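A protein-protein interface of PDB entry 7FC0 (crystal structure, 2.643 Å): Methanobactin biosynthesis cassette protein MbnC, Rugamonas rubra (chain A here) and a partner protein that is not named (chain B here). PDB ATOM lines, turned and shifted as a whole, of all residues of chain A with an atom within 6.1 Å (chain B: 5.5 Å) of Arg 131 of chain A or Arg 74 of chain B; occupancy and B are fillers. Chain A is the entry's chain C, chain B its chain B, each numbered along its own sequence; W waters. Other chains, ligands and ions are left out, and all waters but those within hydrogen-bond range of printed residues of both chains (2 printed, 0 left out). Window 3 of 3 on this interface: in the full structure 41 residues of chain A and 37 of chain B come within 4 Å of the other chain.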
ATOM      1  N   TRP A 126     -28.605  33.469  37.921  1.00  0.00           N
ATOM      2  CA  TRP A 126     -27.289  32.900  37.651  1.00  0.00           C
ATOM      3  C   TRP A 126     -27.414  31.477  37.131  1.00  0.00           C
ATOM      4  O   TRP A 126     -26.727  31.098  36.182  1.00  0.00           O
ATOM      5  CB  TRP A 126     -26.411  32.924  38.909  1.00  0.00           C
ATOM      6  CG  TRP A 126     -25.031  32.323  38.675  1.00  0.00           C
ATOM      7  CD1 TRP A 126     -23.911  32.989  38.282  1.00  0.00           C
ATOM      8  CD2 TRP A 126     -24.655  30.952  38.811  1.00  0.00           C
ATOM      9  NE1 TRP A 126     -22.863  32.120  38.158  1.00  0.00           N
ATOM     10  CE2 TRP A 126     -23.294  30.859  38.474  1.00  0.00           C
ATOM     11  CE3 TRP A 126     -25.340  29.793  39.177  1.00  0.00           C
ATOM     12  CZ2 TRP A 126     -22.592  29.644  38.497  1.00  0.00           C
ATOM     13  CZ3 TRP A 126     -24.649  28.580  39.200  1.00  0.00           C
ATOM     14  CH2 TRP A 126     -23.287  28.517  38.860  1.00  0.00           C
ATOM     15  N   ALA A 127     -28.264  30.672  37.769  1.00  0.00           N
ATOM     16  CA  ALA A 127     -28.426  29.274  37.401  1.00  0.00           C
ATOM     17  C   ALA A 127     -29.009  29.112  36.000  1.00  0.00           C
ATOM     18  O   ALA A 127     -28.751  28.107  35.334  1.00  0.00           O
ATOM     19  CB  ALA A 127     -29.308  28.578  38.447  1.00  0.00           C
ATOM     20  N   VAL A 128     -29.798  30.070  35.540  1.00  0.00           N
ATOM     21  CA  VAL A 128     -30.424  29.948  34.233  1.00  0.00           C
ATOM     22  C   VAL A 128     -29.515  30.480  33.140  1.00  0.00           C
ATOM     23  O   VAL A 128     -29.464  29.923  32.043  1.00  0.00           O
ATOM     24  CB  VAL A 128     -31.788  30.675  34.251  1.00  0.00           C
ATOM     25  CG1 VAL A 128     -32.330  30.944  32.847  1.00  0.00           C
ATOM     26  CG2 VAL A 128     -32.769  29.875  35.018  1.00  0.00           C
ATOM     27  N   LEU A 129     -28.770  31.542  33.424  1.00  0.00           N
ATOM     28  CA  LEU A 129     -28.047  32.248  32.381  1.00  0.00           C
ATOM     29  C   LEU A 129     -26.554  31.950  32.308  1.00  0.00           C
ATOM     30  O   LEU A 129     -25.978  32.078  31.220  1.00  0.00           O
ATOM     31  CB  LEU A 129     -28.231  33.744  32.552  1.00  0.00           C
ATOM     32  CG  LEU A 129     -29.646  34.168  32.212  1.00  0.00           C
ATOM     33  CD1 LEU A 129     -29.716  35.712  32.206  1.00  0.00           C
ATOM     34  CD2 LEU A 129     -30.096  33.523  30.889  1.00  0.00           C
ATOM     35  N   ASP A 130     -25.918  31.572  33.417  1.00  0.00           N
ATOM     36  CA  ASP A 130     -24.470  31.370  33.441  1.00  0.00           C
ATOM     37  C   ASP A 130     -24.042  30.179  32.593  1.00  0.00           C
ATOM     38  O   ASP A 130     -24.651  29.112  32.639  1.00  0.00           O
ATOM     39  CB  ASP A 130     -23.975  31.173  34.877  1.00  0.00           C
ATOM     40  CG  ASP A 130     -22.481  30.943  34.952  1.00  0.00           C
ATOM     41  OD1 ASP A 130     -21.716  31.930  34.960  1.00  0.00           O
ATOM     42  OD2 ASP A 130     -22.077  29.771  34.993  1.00  0.00           O
ATOM     43  N   ARG A 131     -22.955  30.355  31.851  1.00  0.00           N
ATOM     44  CA  ARG A 131     -22.487  29.346  30.910  1.00  0.00           C
ATOM     45  C   ARG A 131     -21.061  28.898  31.205  1.00  0.00           C
ATOM     46  O   ARG A 131     -20.339  28.459  30.316  1.00  0.00           O
ATOM     47  CB  ARG A 131     -22.615  29.871  29.485  1.00  0.00           C
ATOM     48  CG  ARG A 131     -24.058  29.985  29.049  1.00  0.00           C
ATOM     49  CD  ARG A 131     -24.665  28.621  29.028  1.00  0.00           C
ATOM     50  NE  ARG A 131     -25.996  28.670  28.469  1.00  0.00           N
ATOM     51  CZ  ARG A 131     -27.074  28.845  29.206  1.00  0.00           C
ATOM     52  NH1 ARG A 131     -26.937  28.978  30.519  1.00  0.00           N
ATOM     53  NH2 ARG A 131     -28.271  28.880  28.641  1.00  0.00           N
ATOM     54  N   SER A 132     -20.651  29.001  32.448  1.00  0.00           N
ATOM     55  CA  SER A 132     -19.359  28.519  32.878  1.00  0.00           C
ATOM     56  C   SER A 132     -19.475  27.069  33.330  1.00  0.00           C
ATOM     57  O   SER A 132     -20.564  26.512  33.408  1.00  0.00           O
ATOM     58  CB  SER A 132     -18.843  29.367  34.029  1.00  0.00           C
ATOM     59  OG  SER A 132     -19.386  28.862  35.236  1.00  0.00           O
ATOM     60  N   ALA A 133     -18.346  26.471  33.711  1.00  0.00           N
ATOM     61  CA  ALA A 133     -18.380  25.097  34.189  1.00  0.00           C
ATOM     62  C   ALA A 133     -18.950  24.961  35.594  1.00  0.00           C
ATOM     63  O   ALA A 133     -19.161  23.833  36.043  1.00  0.00           O
ATOM     64  CB  ALA A 133     -16.986  24.486  34.143  1.00  0.00           C
ATOM     65  N   LYS A 152     -27.805  25.021  39.061  1.00  0.00           N
ATOM     66  CA  LYS A 152     -28.149  24.660  37.697  1.00  0.00           C
ATOM     67  C   LYS A 152     -28.790  23.273  37.662  1.00  0.00           C
ATOM     68  O   LYS A 152     -28.419  22.393  38.444  1.00  0.00           O
ATOM     69  CB  LYS A 152     -26.902  24.659  36.820  1.00  0.00           C
ATOM     70  CG  LYS A 152     -26.434  26.044  36.413  1.00  0.00           C
ATOM     71  CD  LYS A 152     -25.084  25.942  35.739  1.00  0.00           C
ATOM     72  CE  LYS A 152     -24.608  27.282  35.240  1.00  0.00           C
ATOM     73  NZ  LYS A 152     -23.216  27.152  34.719  1.00  0.00           N
ATOM     74  N   ASP B  33     -27.389  24.381  25.172  1.00  0.00           N
ATOM     75  CA  ASP B  33     -26.645  24.931  26.307  1.00  0.00           C
ATOM     76  C   ASP B  33     -27.512  25.138  27.535  1.00  0.00           C
ATOM     77  O   ASP B  33     -26.995  25.584  28.562  1.00  0.00           O
ATOM     78  CB  ASP B  33     -25.891  26.222  25.944  1.00  0.00           C
ATOM     79  CG  ASP B  33     -26.785  27.327  25.444  1.00  0.00           C
ATOM     80  OD1 ASP B  33     -27.594  27.064  24.528  1.00  0.00           O
ATOM     81  OD2 ASP B  33     -26.631  28.472  25.928  1.00  0.00           O
ATOM     82  N   ASN B  34     -28.749  24.681  27.518  1.00  0.00           N
ATOM     83  CA  ASN B  34     -29.557  24.747  28.752  1.00  0.00           C
ATOM     84  C   ASN B  34     -29.391  23.438  29.511  1.00  0.00           C
ATOM     85  O   ASN B  34     -29.886  23.367  30.620  1.00  0.00           O
ATOM     86  CB  ASN B  34     -31.030  25.044  28.495  1.00  0.00           C
ATOM     87  CG  ASN B  34     -31.323  26.382  27.864  1.00  0.00           C
ATOM     88  OD1 ASN B  34     -32.480  26.742  27.709  1.00  0.00           O
ATOM     89  ND2 ASN B  34     -30.295  27.116  27.491  1.00  0.00           N
ATOM     90  N   MET B  36     -26.242  21.636  29.849  1.00  0.00           N
ATOM     91  CA  MET B  36     -24.844  21.270  29.904  1.00  0.00           C
ATOM     92  C   MET B  36     -24.385  20.833  31.280  1.00  0.00           C
ATOM     93  O   MET B  36     -23.184  20.582  31.450  1.00  0.00           O
ATOM     94  CB  MET B  36     -23.994  22.449  29.426  1.00  0.00           C
ATOM     95  CG  MET B  36     -24.098  22.626  27.929  1.00  0.00           C
ATOM     96  SD  MET B  36     -23.102  23.976  27.362  1.00  0.00           S
ATOM     97  CE  MET B  36     -21.477  23.487  27.920  1.00  0.00           C
ATOM     98  N   GLN B  37     -25.293  20.711  32.248  1.00  0.00           N
ATOM     99  CA  GLN B  37     -24.999  20.013  33.494  1.00  0.00           C
ATOM    100  C   GLN B  37     -25.798  18.724  33.627  1.00  0.00           C
ATOM    101  O   GLN B  37     -25.604  17.982  34.598  1.00  0.00           O
ATOM    102  CB  GLN B  37     -25.246  20.929  34.701  1.00  0.00           C
ATOM    103  CG  GLN B  37     -24.695  22.360  34.538  1.00  0.00           C
ATOM    104  CD  GLN B  37     -23.210  22.426  34.147  1.00  0.00           C
ATOM    105  OE1 GLN B  37     -22.395  21.564  34.519  1.00  0.00           O
ATOM    106  NE2 GLN B  37     -22.856  23.473  33.407  1.00  0.00           N
ATOM    107  N   MET B  56     -28.013  28.903  22.491  1.00  0.00           N
ATOM    108  CA  MET B  56     -28.457  30.254  22.788  1.00  0.00           C
ATOM    109  C   MET B  56     -27.328  31.216  23.126  1.00  0.00           C
ATOM    110  O   MET B  56     -27.276  32.303  22.557  1.00  0.00           O
ATOM    111  CB  MET B  56     -29.461  30.226  23.950  1.00  0.00           C
ATOM    112  CG  MET B  56     -30.031  31.581  24.302  1.00  0.00           C
ATOM    113  SD  MET B  56     -31.190  32.128  23.056  1.00  0.00           S
ATOM    114  CE  MET B  56     -30.262  33.350  22.133  1.00  0.00           C
ATOM    115  N   PHE B  57     -26.375  30.829  23.964  1.00  0.00           N
ATOM    116  CA  PHE B  57     -25.444  31.799  24.529  1.00  0.00           C
ATOM    117  C   PHE B  57     -23.988  31.436  24.286  1.00  0.00           C
ATOM    118  O   PHE B  57     -23.151  31.556  25.184  1.00  0.00           O
ATOM    119  CB  PHE B  57     -25.689  31.966  26.020  1.00  0.00           C
ATOM    120  CG  PHE B  57     -26.943  32.697  26.347  1.00  0.00           C
ATOM    121  CD1 PHE B  57     -27.091  34.036  26.013  1.00  0.00           C
ATOM    122  CD2 PHE B  57     -27.978  32.057  27.024  1.00  0.00           C
ATOM    123  CE1 PHE B  57     -28.266  34.731  26.343  1.00  0.00           C
ATOM    124  CE2 PHE B  57     -29.143  32.742  27.361  1.00  0.00           C
ATOM    125  CZ  PHE B  57     -29.291  34.077  27.020  1.00  0.00           C
ATOM    126  N   ARG B  69     -13.294  28.883  23.599  1.00  0.00           N
ATOM    127  CA  ARG B  69     -12.648  27.588  23.475  1.00  0.00           C
ATOM    128  C   ARG B  69     -13.118  26.638  24.570  1.00  0.00           C
ATOM    129  O   ARG B  69     -13.389  25.463  24.295  1.00  0.00           O
ATOM    130  CB  ARG B  69     -11.126  27.769  23.504  1.00  0.00           C
ATOM    131  CG  ARG B  69     -10.614  28.717  22.412  1.00  0.00           C
ATOM    132  CD  ARG B  69      -9.104  28.827  22.295  1.00  0.00           C
ATOM    133  NE  ARG B  69      -8.642  28.015  21.167  1.00  0.00           N
ATOM    134  CZ  ARG B  69      -8.217  28.500  20.001  1.00  0.00           C
ATOM    135  NH1 ARG B  69      -8.187  29.815  19.795  1.00  0.00           N
ATOM    136  NH2 ARG B  69      -7.816  27.662  19.041  1.00  0.00           N
ATOM    137  N   ASP B  70     -13.280  27.138  25.799  1.00  0.00           N
ATOM    138  CA  ASP B  70     -13.779  26.297  26.884  1.00  0.00           C
ATOM    139  C   ASP B  70     -15.237  25.900  26.679  1.00  0.00           C
ATOM    140  O   ASP B  70     -15.634  24.782  27.015  1.00  0.00           O
ATOM    141  CB  ASP B  70     -13.637  27.005  28.224  1.00  0.00           C
ATOM    142  CG  ASP B  70     -14.229  26.191  29.361  1.00  0.00           C
ATOM    143  OD1 ASP B  70     -13.634  25.155  29.736  1.00  0.00           O
ATOM    144  OD2 ASP B  70     -15.319  26.560  29.848  1.00  0.00           O
ATOM    145  N   PHE B  71     -16.063  26.818  26.187  1.00  0.00           N
ATOM    146  CA  PHE B  71     -17.438  26.465  25.876  1.00  0.00           C
ATOM    147  C   PHE B  71     -17.473  25.340  24.852  1.00  0.00           C
ATOM    148  O   PHE B  71     -18.210  24.364  25.008  1.00  0.00           O
ATOM    149  CB  PHE B  71     -18.173  27.700  25.369  1.00  0.00           C
ATOM    150  CG  PHE B  71     -19.660  27.544  25.258  1.00  0.00           C
ATOM    151  CD1 PHE B  71     -20.466  27.608  26.382  1.00  0.00           C
ATOM    152  CD2 PHE B  71     -20.257  27.398  24.026  1.00  0.00           C
ATOM    153  CE1 PHE B  71     -21.845  27.499  26.278  1.00  0.00           C
ATOM    154  CE2 PHE B  71     -21.631  27.286  23.922  1.00  0.00           C
ATOM    155  CZ  PHE B  71     -22.427  27.346  25.057  1.00  0.00           C
ATOM    156  N   ALA B  72     -16.658  25.454  23.802  1.00  0.00           N
ATOM    157  CA  ALA B  72     -16.573  24.392  22.812  1.00  0.00           C
ATOM    158  C   ALA B  72     -16.123  23.072  23.440  1.00  0.00           C
ATOM    159  O   ALA B  72     -16.722  22.022  23.188  1.00  0.00           O
ATOM    160  CB  ALA B  72     -15.626  24.813  21.687  1.00  0.00           C
ATOM    161  N   ALA B  73     -15.090  23.102  24.273  1.00  0.00           N
ATOM    162  CA  ALA B  73     -14.609  21.868  24.886  1.00  0.00           C
ATOM    163  C   ALA B  73     -15.703  21.182  25.690  1.00  0.00           C
ATOM    164  O   ALA B  73     -15.800  19.949  25.696  1.00  0.00           O
ATOM    165  CB  ALA B  73     -13.394  22.145  25.762  1.00  0.00           C
ATOM    166  N   ARG B  74     -16.527  21.958  26.390  1.00  0.00           N
ATOM    167  CA  ARG B  74     -17.546  21.364  27.242  1.00  0.00           C
ATOM    168  C   ARG B  74     -18.772  20.930  26.456  1.00  0.00           C
ATOM    169  O   ARG B  74     -19.554  20.112  26.933  1.00  0.00           O
ATOM    170  CB  ARG B  74     -17.898  22.352  28.353  1.00  0.00           C
ATOM    171  CG  ARG B  74     -16.700  22.630  29.235  1.00  0.00           C
ATOM    172  CD  ARG B  74     -16.987  23.451  30.457  1.00  0.00           C
ATOM    173  NE  ARG B  74     -18.333  23.986  30.433  1.00  0.00           N
ATOM    174  CZ  ARG B  74     -18.626  25.244  30.160  1.00  0.00           C
ATOM    175  NH1 ARG B  74     -17.660  26.101  29.876  1.00  0.00           N
ATOM    176  NH2 ARG B  74     -19.891  25.632  30.175  1.00  0.00           N
ATOM    177  N   LEU B  75     -18.920  21.421  25.248  1.00  0.00           N
ATOM    178  CA  LEU B  75     -20.071  21.126  24.450  1.00  0.00           C
ATOM    179  C   LEU B  75     -19.815  19.968  23.508  1.00  0.00           C
ATOM    180  O   LEU B  75     -20.768  19.321  23.072  1.00  0.00           O
ATOM    181  CB  LEU B  75     -20.470  22.386  23.682  1.00  0.00           C
ATOM    182  CG  LEU B  75     -21.769  22.379  22.903  1.00  0.00           C
ATOM    183  CD1 LEU B  75     -22.906  22.201  23.866  1.00  0.00           C
ATOM    184  CD2 LEU B  75     -21.881  23.700  22.182  1.00  0.00           C
ATOM    185  N   ARG B  76     -18.551  19.686  23.211  1.00  0.00           N
ATOM    186  CA  ARG B  76     -18.230  18.566  22.333  1.00  0.00           C
ATOM    187  C   ARG B  76     -18.685  17.222  22.882  1.00  0.00           C
ATOM    188  O   ARG B  76     -19.155  16.396  22.083  1.00  0.00           O
ATOM    189  CB  ARG B  76     -16.722  18.531  22.060  1.00  0.00           C
ATOM    190  CG  ARG B  76     -16.231  19.311  20.845  1.00  0.00           C
ATOM    191  CD  ARG B  76     -14.758  18.998  20.677  1.00  0.00           C
ATOM    192  NE  ARG B  76     -14.129  19.608  19.504  1.00  0.00           N
ATOM    193  CZ  ARG B  76     -13.586  18.920  18.495  1.00  0.00           C
ATOM    194  NH1 ARG B  76     -13.599  17.590  18.513  1.00  0.00           N
ATOM    195  NH2 ARG B  76     -13.024  19.560  17.468  1.00  0.00           N
ATOM    196  N   PRO B  77     -18.603  16.930  24.183  1.00  0.00           N
ATOM    197  CA  PRO B  77     -19.133  15.643  24.648  1.00  0.00           C
ATOM    198  C   PRO B  77     -20.593  15.442  24.321  1.00  0.00           C
ATOM    199  O   PRO B  77     -21.004  14.301  24.074  1.00  0.00           O
ATOM    200  CB  PRO B  77     -18.898  15.701  26.162  1.00  0.00           C
ATOM    201  CG  PRO B  77     -17.725  16.513  26.287  1.00  0.00           C
ATOM    202  CD  PRO B  77     -17.882  17.607  25.270  1.00  0.00           C
ATOM    203  N   TYR B  78     -21.379  16.523  24.270  1.00  0.00           N
ATOM    204  CA  TYR B  78     -22.795  16.395  23.932  1.00  0.00           C
ATOM    205  C   TYR B  78     -23.004  16.104  22.459  1.00  0.00           C
ATOM    206  O   TYR B  78     -23.965  15.415  22.108  1.00  0.00           O
ATOM    207  CB  TYR B  78     -23.557  17.656  24.309  1.00  0.00           C
ATOM    208  CG  TYR B  78     -23.720  17.768  25.774  1.00  0.00           C
ATOM    209  CD1 TYR B  78     -22.721  18.346  26.543  1.00  0.00           C
ATOM    210  CD2 TYR B  78     -24.848  17.271  26.415  1.00  0.00           C
ATOM    211  CE1 TYR B  78     -22.848  18.463  27.910  1.00  0.00           C
ATOM    212  CE2 TYR B  78     -24.974  17.379  27.807  1.00  0.00           C
ATOM    213  CZ  TYR B  78     -23.956  17.974  28.537  1.00  0.00           C
ATOM    214  OH  TYR B  78     -24.017  18.100  29.891  1.00  0.00           O
HETATM  215  O   HOH W   1     -22.535  26.040  30.011  1.00  0.00           O
HETATM  216  O   HOH W   2     -24.011  25.921  32.396  1.00  0.00           O
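Water W1 lies within hydrogen-bond range of NH2 of Arg 74 of chain B (2.7 Å), O of Arg 131 of chain A (3.3 Å) and SD of Met 36 of chain B (3.4 Å). Water W2 lies within hydrogen-bond range of NZ of Lys 152 of chain A, NE2 of Gln 37 of chain B and O of Asp 130 of chain A.
The backbone carbonyl oxygen of Val 128 of chain A sits at hydrogen-bond distance from the guanidinium group of Arg 131 of chain A. NZ of Lys 152 of chain A lies within hydrogen-bond range of O of Ser 132 of chain A, at 3.0 Å. The guanidinium group (NH1) of Arg 131 of chain A sits at hydrogen-bond distance from the backbone carbonyl oxygen (O) of Leu 129 of chain A. The side-chain carboxylate (OD1) of Asp 33 of chain B sits at hydrogen-bond distance from the backbone NH (N) of Met 56 of chain B. The side-chain hydroxyl (OG) of Ser 132 of chain A is in hydrogen-bond range of the side-chain carboxylate (OD2) of Asp 130 of chain A, at 2.9 Å. OD2 of Asp 130 of chain A lies within salt-bridge range of NZ of Lys 152 of chain A (2.9 Å).
Among the printed residues, pairs that only touch across the chains: Arg 131 of chain A with Phe 57 of chain B, Leu 129 of chain A with Phe 57 of chain B, Ala 133 of chain A with Arg 74 of chain B, Lys 152 of chain A with Gln 37 of chain B and Ser 132 of chain A with Gln 37 of chain B.
Of the 9 printed residues of chain A, 5 touch a printed residue of chain B. Hydrophobic or aromatic side chains of chain A that line the printed part of chain B: Leu 129 and Ala 133. Along chain A the printed residues that touch a printed residue of chain B span positions 129 to 152. Of the 16 printed residues of chain B, 5 touch a printed residue of chain A. Along chain B the printed residues that touch a printed residue of chain A span positions 33 to 74. Among the printed residues, 9 pairs touch across the chains. Among the printed residues, Asp or Glu carboxylates within 4 Å of a Lys or Arg side-chain nitrogen of the other chain: Arg 131 of chain A with Asp 33 of chain B (2.6 Å).
The side-chain amide nitrogen (ND2) of Asn 34 of chain B sits close to the guanidinium group (NH2) of Arg 131 of chain A, at 2.9 Å. The guanidinium group (NH2) of Arg 74 of chain B sits at hydrogen-bond distance from the backbone carbonyl oxygen (O) of Ser 132 of chain A (3.4 Å). The guanidinium group (NE) of Arg 131 of chain A is in salt-bridge range of the side-chain carboxylate (OD2) of Asp 33 of chain B (2.6 Å). The backbone carbonyl oxygen of Arg 131 of chain A is in hydrogen-bond range of the guanidinium group of Arg 74 of chain B, 2.9 Å away.
Trp 126 of chain A touches none of the printed residues of chain B. Of the printed residues of chain B, Leu 129 of chain A touches Phe 57. Arg 131 of chain A touches just these residues of chain B: Asp 33, Asn 34, Phe 57 and Arg 74. Of the printed residues of chain B, Ser 132 of chain A touches Gln 37 (3.8 Å) and Arg 74 (3.4 Å). Of the printed residues of chain B, Lys 152 of chain A touches Gln 37 (3.8 Å). Of the printed residues of chain A, Asp 33 of chain B touches Arg 131. Printed residues of chain A within 4 Å of Gln 37 of chain B: Ser 132 and Lys 152. Ala 73 of chain B touches none of the printed residues of chain A. The nearest residue of chain B that does not touch Arg 131 of chain A is Phe 71 of chain B (4.03 Å). The nearest printed residue of chain B that does not touch Ala 133 of chain A is Gln 37 of chain B (4.2 Å).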
